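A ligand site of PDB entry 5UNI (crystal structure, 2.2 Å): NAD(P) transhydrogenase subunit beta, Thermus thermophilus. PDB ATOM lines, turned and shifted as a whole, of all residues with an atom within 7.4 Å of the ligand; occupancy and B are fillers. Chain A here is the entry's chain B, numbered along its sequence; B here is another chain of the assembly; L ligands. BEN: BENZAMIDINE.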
ATOM      1  N   TRP A  49      18.841 -23.621 -14.038  1.00  0.00           N
ATOM      2  CA  TRP A  49      17.906 -22.653 -14.632  1.00  0.00           C
ATOM      3  C   TRP A  49      17.017 -22.028 -13.524  1.00  0.00           C
ATOM      4  O   TRP A  49      16.625 -22.729 -12.594  1.00  0.00           O
ATOM      5  CB  TRP A  49      17.071 -23.379 -15.681  1.00  0.00           C
ATOM      6  CG  TRP A  49      16.272 -22.536 -16.550  1.00  0.00           C
ATOM      7  CD1 TRP A  49      15.121 -21.916 -16.230  1.00  0.00           C
ATOM      8  CD2 TRP A  49      16.471 -22.325 -17.949  1.00  0.00           C
ATOM      9  NE1 TRP A  49      14.606 -21.273 -17.317  1.00  0.00           N
ATOM     10  CE2 TRP A  49      15.417 -21.502 -18.391  1.00  0.00           C
ATOM     11  CE3 TRP A  49      17.467 -22.701 -18.850  1.00  0.00           C
ATOM     12  CZ2 TRP A  49      15.311 -21.052 -19.695  1.00  0.00           C
ATOM     13  CZ3 TRP A  49      17.355 -22.266 -20.143  1.00  0.00           C
ATOM     14  CH2 TRP A  49      16.297 -21.426 -20.559  1.00  0.00           C
ATOM     15  N   GLU A 103       3.320 -25.980 -23.577  1.00  0.00           N
ATOM     16  CA  GLU A 103       3.311 -24.529 -23.620  1.00  0.00           C
ATOM     17  C   GLU A 103       2.008 -24.035 -24.219  1.00  0.00           C
ATOM     18  O   GLU A 103       1.551 -22.984 -23.851  1.00  0.00           O
ATOM     19  CB  GLU A 103       4.505 -23.961 -24.416  1.00  0.00           C
ATOM     20  CG  GLU A 103       5.870 -24.419 -23.941  1.00  0.00           C
ATOM     21  CD  GLU A 103       6.321 -23.804 -22.632  1.00  0.00           C
ATOM     22  OE1 GLU A 103       7.439 -23.242 -22.601  1.00  0.00           O
ATOM     23  OE2 GLU A 103       5.599 -23.916 -21.616  1.00  0.00           O
ATOM     24  N   LYS A 106      -0.579 -24.554 -21.270  1.00  0.00           N
ATOM     25  CA  LYS A 106      -0.410 -23.432 -20.336  1.00  0.00           C
ATOM     26  C   LYS A 106      -0.882 -22.090 -20.881  1.00  0.00           C
ATOM     27  O   LYS A 106      -1.002 -21.173 -20.088  1.00  0.00           O
ATOM     28  CB  LYS A 106       1.073 -23.193 -19.948  1.00  0.00           C
ATOM     29  CG  LYS A 106       1.656 -24.231 -19.034  1.00  0.00           C
ATOM     30  CD  LYS A 106       2.951 -23.765 -18.375  1.00  0.00           C
ATOM     31  CE  LYS A 106       3.271 -24.652 -17.173  1.00  0.00           C
ATOM     32  NZ  LYS A 106       4.378 -24.089 -16.367  1.00  0.00           N
ATOM     33  N   GLY A 107      -1.102 -21.946 -22.198  1.00  0.00           N
ATOM     34  CA  GLY A 107      -1.301 -20.638 -22.787  1.00  0.00           C
ATOM     35  C   GLY A 107      -0.116 -19.692 -22.514  1.00  0.00           C
ATOM     36  O   GLY A 107      -0.309 -18.511 -22.266  1.00  0.00           O
ATOM     37  N   ALA A 108       1.114 -20.215 -22.587  1.00  0.00           N
ATOM     38  CA  ALA A 108       2.315 -19.477 -22.168  1.00  0.00           C
ATOM     39  C   ALA A 108       2.739 -18.339 -23.134  1.00  0.00           C
ATOM     40  O   ALA A 108       3.526 -17.511 -22.752  1.00  0.00           O
ATOM     41  CB  ALA A 108       3.486 -20.455 -21.943  1.00  0.00           C
ATOM     42  N   PHE A 109       2.209 -18.300 -24.355  1.00  0.00           N
ATOM     43  CA  PHE A 109       2.652 -17.328 -25.356  1.00  0.00           C
ATOM     44  C   PHE A 109       1.778 -16.095 -25.359  1.00  0.00           C
ATOM     45  O   PHE A 109       0.599 -16.217 -25.622  1.00  0.00           O
ATOM     46  CB  PHE A 109       2.627 -17.969 -26.750  1.00  0.00           C
ATOM     47  CG  PHE A 109       3.489 -19.200 -26.844  1.00  0.00           C
ATOM     48  CD1 PHE A 109       4.866 -19.085 -26.890  1.00  0.00           C
ATOM     49  CD2 PHE A 109       2.928 -20.461 -26.880  1.00  0.00           C
ATOM     50  CE1 PHE A 109       5.663 -20.196 -26.985  1.00  0.00           C
ATOM     51  CE2 PHE A 109       3.728 -21.588 -26.959  1.00  0.00           C
ATOM     52  CZ  PHE A 109       5.090 -21.453 -27.002  1.00  0.00           C
ATOM     53  N   GLU A 110       2.350 -14.926 -25.060  1.00  0.00           N
ATOM     54  CA  GLU A 110       1.630 -13.650 -25.206  1.00  0.00           C
ATOM     55  C   GLU A 110       1.745 -13.165 -26.647  1.00  0.00           C
ATOM     56  O   GLU A 110       0.828 -12.560 -27.180  1.00  0.00           O
ATOM     57  CB  GLU A 110       2.141 -12.592 -24.214  1.00  0.00           C
ATOM     58  N   LEU A 114       5.580 -16.050 -31.682  1.00  0.00           N
ATOM     59  CA  LEU A 114       6.237 -17.106 -30.927  1.00  0.00           C
ATOM     60  C   LEU A 114       5.333 -18.323 -30.825  1.00  0.00           C
ATOM     61  O   LEU A 114       5.840 -19.459 -30.746  1.00  0.00           O
ATOM     62  CB  LEU A 114       6.665 -16.659 -29.545  1.00  0.00           C
ATOM     63  CG  LEU A 114       7.685 -15.509 -29.425  1.00  0.00           C
ATOM     64  CD1 LEU A 114       7.816 -15.113 -27.971  1.00  0.00           C
ATOM     65  CD2 LEU A 114       9.012 -15.897 -30.040  1.00  0.00           C
ATOM     66  N   GLU A 221      11.263 -24.874 -31.541  1.00  0.00           N
ATOM     67  CA  GLU A 221      10.863 -24.833 -30.124  1.00  0.00           C
ATOM     68  C   GLU A 221      11.804 -23.922 -29.345  1.00  0.00           C
ATOM     69  O   GLU A 221      11.350 -23.102 -28.493  1.00  0.00           O
ATOM     70  CB  GLU A 221      10.694 -26.240 -29.497  1.00  0.00           C
ATOM     71  CG  GLU A 221       9.617 -27.110 -30.149  1.00  0.00           C
ATOM     72  CD  GLU A 221       8.235 -26.448 -30.265  1.00  0.00           C
ATOM     73  OE1 GLU A 221       7.624 -26.557 -31.336  1.00  0.00           O
ATOM     74  OE2 GLU A 221       7.739 -25.794 -29.327  1.00  0.00           O
ATOM     75  N   GLY A 222      13.070 -23.993 -29.715  1.00  0.00           N
ATOM     76  CA  GLY A 222      14.106 -23.140 -29.147  1.00  0.00           C
ATOM     77  C   GLY A 222      13.835 -21.661 -29.282  1.00  0.00           C
ATOM     78  O   GLY A 222      13.930 -20.932 -28.305  1.00  0.00           O
ATOM     79  N   PHE A 223      13.529 -21.215 -30.505  1.00  0.00           N
ATOM     80  CA  PHE A 223      13.204 -19.818 -30.737  1.00  0.00           C
ATOM     81  C   PHE A 223      11.897 -19.443 -29.979  1.00  0.00           C
ATOM     82  O   PHE A 223      11.811 -18.374 -29.430  1.00  0.00           O
ATOM     83  CB  PHE A 223      13.070 -19.508 -32.232  1.00  0.00           C
ATOM     84  CG  PHE A 223      14.371 -19.511 -32.918  1.00  0.00           C
ATOM     85  CD1 PHE A 223      15.290 -18.497 -32.657  1.00  0.00           C
ATOM     86  CD2 PHE A 223      14.733 -20.550 -33.772  1.00  0.00           C
ATOM     87  CE1 PHE A 223      16.571 -18.531 -33.210  1.00  0.00           C
ATOM     88  CE2 PHE A 223      16.015 -20.597 -34.344  1.00  0.00           C
ATOM     89  CZ  PHE A 223      16.920 -19.564 -34.063  1.00  0.00           C
ATOM     90  N   ALA A 224      10.894 -20.332 -29.976  1.00  0.00           N
ATOM     91  CA  ALA A 224       9.594 -20.048 -29.356  1.00  0.00           C
ATOM     92  C   ALA A 224       9.694 -19.870 -27.850  1.00  0.00           C
ATOM     93  O   ALA A 224       9.030 -18.999 -27.313  1.00  0.00           O
ATOM     94  CB  ALA A 224       8.597 -21.184 -29.651  1.00  0.00           C
ATOM     95  N   VAL A 225      10.476 -20.728 -27.185  1.00  0.00           N
ATOM     96  CA  VAL A 225      10.670 -20.626 -25.730  1.00  0.00           C
ATOM     97  C   VAL A 225      11.940 -19.850 -25.313  1.00  0.00           C
ATOM     98  O   VAL A 225      12.126 -19.658 -24.163  1.00  0.00           O
ATOM     99  CB  VAL A 225      10.708 -22.001 -25.024  1.00  0.00           C
ATOM    100  CG1 VAL A 225       9.591 -22.887 -25.512  1.00  0.00           C
ATOM    101  CG2 VAL A 225      12.033 -22.732 -25.254  1.00  0.00           C
ATOM    102  N   GLY A 226      12.792 -19.416 -26.244  1.00  0.00           N
ATOM    103  CA  GLY A 226      14.024 -18.649 -25.859  1.00  0.00           C
ATOM    104  C   GLY A 226      15.112 -19.513 -25.197  1.00  0.00           C
ATOM    105  O   GLY A 226      15.652 -19.136 -24.169  1.00  0.00           O
ATOM    106  N   ASN A 227      15.386 -20.689 -25.737  1.00  0.00           N
ATOM    107  CA  ASN A 227      16.514 -21.504 -25.341  1.00  0.00           C
ATOM    108  C   ASN A 227      17.575 -21.606 -26.453  1.00  0.00           C
ATOM    109  O   ASN A 227      17.327 -22.321 -27.469  1.00  0.00           O
ATOM    110  CB  ASN A 227      16.083 -22.897 -24.941  1.00  0.00           C
ATOM    111  CG  ASN A 227      17.244 -23.694 -24.348  1.00  0.00           C
ATOM    112  OD1 ASN A 227      18.360 -23.686 -24.884  1.00  0.00           O
ATOM    113  ND2 ASN A 227      17.004 -24.334 -23.209  1.00  0.00           N
ATOM    114  N   MET B   1      16.103 -15.938 -20.441  1.00  0.00           N
ATOM    115  CA  MET B   1      17.169 -16.362 -21.416  1.00  0.00           C
ATOM    116  C   MET B   1      16.921 -16.031 -22.900  1.00  0.00           C
ATOM    117  O   MET B   1      17.643 -16.501 -23.764  1.00  0.00           O
ATOM    118  CB  MET B   1      17.408 -17.869 -21.322  1.00  0.00           C
ATOM    119  CG  MET B   1      18.709 -18.317 -21.947  1.00  0.00           C
ATOM    120  SD  MET B   1      19.626 -19.549 -20.987  1.00  0.00           S
ATOM    121  CE  MET B   1      19.726 -18.736 -19.384  1.00  0.00           C
ATOM    122  N   GLU B   2      15.916 -15.212 -23.189  1.00  0.00           N
ATOM    123  CA  GLU B   2      15.593 -14.781 -24.558  1.00  0.00           C
ATOM    124  C   GLU B   2      16.586 -13.686 -25.087  1.00  0.00           C
ATOM    125  O   GLU B   2      17.061 -12.851 -24.323  1.00  0.00           O
ATOM    126  CB  GLU B   2      14.145 -14.275 -24.567  1.00  0.00           C
ATOM    127  CG  GLU B   2      13.565 -13.926 -25.928  1.00  0.00           C
ATOM    128  CD  GLU B   2      12.042 -13.837 -25.948  1.00  0.00           C
ATOM    129  OE1 GLU B   2      11.400 -13.738 -24.871  1.00  0.00           O
ATOM    130  OE2 GLU B   2      11.466 -13.864 -27.067  1.00  0.00           O
ATOM    131  N   VAL B  51      13.466 -28.097 -18.764  1.00  0.00           N
ATOM    132  CA  VAL B  51      12.955 -26.785 -18.289  1.00  0.00           C
ATOM    133  C   VAL B  51      11.423 -26.870 -18.163  1.00  0.00           C
ATOM    134  O   VAL B  51      10.828 -26.354 -17.183  1.00  0.00           O
ATOM    135  CB  VAL B  51      13.346 -25.604 -19.225  1.00  0.00           C
ATOM    136  CG1 VAL B  51      12.662 -24.287 -18.794  1.00  0.00           C
ATOM    137  CG2 VAL B  51      14.837 -25.418 -19.274  1.00  0.00           C
ATOM    138  N   VAL B  52      10.778 -27.506 -19.167  1.00  0.00           N
ATOM    139  CA  VAL B  52       9.335 -27.756 -19.076  1.00  0.00           C
ATOM    140  C   VAL B  52       8.981 -28.572 -17.828  1.00  0.00           C
ATOM    141  O   VAL B  52       8.151 -28.170 -17.049  1.00  0.00           O
ATOM    142  CB  VAL B  52       8.800 -28.413 -20.359  1.00  0.00           C
ATOM    143  CG1 VAL B  52       7.377 -28.874 -20.144  1.00  0.00           C
ATOM    144  CG2 VAL B  52       8.881 -27.411 -21.519  1.00  0.00           C
ATOM    145  N   HIS B  55       9.301 -26.496 -14.612  1.00  0.00           N
ATOM    146  CA  HIS B  55       8.299 -25.452 -14.327  1.00  0.00           C
ATOM    147  C   HIS B  55       6.856 -25.983 -14.287  1.00  0.00           C
ATOM    148  O   HIS B  55       5.901 -25.248 -14.070  1.00  0.00           O
ATOM    149  CB  HIS B  55       8.405 -24.331 -15.367  1.00  0.00           C
ATOM    150  CG  HIS B  55       9.644 -23.505 -15.250  1.00  0.00           C
ATOM    151  ND1 HIS B  55      10.301 -22.992 -16.332  1.00  0.00           N
ATOM    152  CD2 HIS B  55      10.342 -23.101 -14.157  1.00  0.00           C
ATOM    153  CE1 HIS B  55      11.356 -22.307 -15.917  1.00  0.00           C
ATOM    154  NE2 HIS B  55      11.414 -22.378 -14.607  1.00  0.00           N
HETATM  155  C1  BEN L   1       8.839 -18.357 -23.328  1.00  0.00           C
HETATM  156  C2  BEN L   1       7.548 -18.417 -23.895  1.00  0.00           C
HETATM  157  C3  BEN L   1       6.629 -19.400 -23.460  1.00  0.00           C
HETATM  158  C4  BEN L   1       6.985 -20.302 -22.472  1.00  0.00           C
HETATM  159  C5  BEN L   1       8.276 -20.264 -21.902  1.00  0.00           C
HETATM  160  C6  BEN L   1       9.196 -19.283 -22.319  1.00  0.00           C
HETATM  161  C   BEN L   1       9.824 -17.310 -23.820  1.00  0.00           C
HETATM  162  N1  BEN L   1      10.613 -16.748 -23.028  1.00  0.00           N
HETATM  163  N2  BEN L   1       9.915 -16.978 -25.129  1.00  0.00           N
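O of Ala 224 lies within hydrogen-bond range of N2 of the ligand.
A nitrogen (N2) of the ligand lies within salt-bridge range of the side-chain carboxylate (OE1) of Glu 2 of chain B (3.6 Å).
O of Val 225 lies close to N1 of the ligand, 3.5 Å away.
O of Glu 103 is in hydrogen-bond range of N of Ala 108 (3.1 Å).
Glu 103 touches the ligand.
CB of Ala 108 touches C4 of the ligand (3.5 Å).
Phe 109 touches the ligand.
Leu 114 touches the ligand.
Gly 226 touches the ligand.
Hydrophobic or aromatic side chains that line the ligand: Ala 108, Phe 109 and Leu 114.
Eight residues have an atom within 4 Å of the ligand: Glu 103, Ala 108, Phe 109, Leu 114, Ala 224, Val 225, Gly 226 and Glu 2 of chain B.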
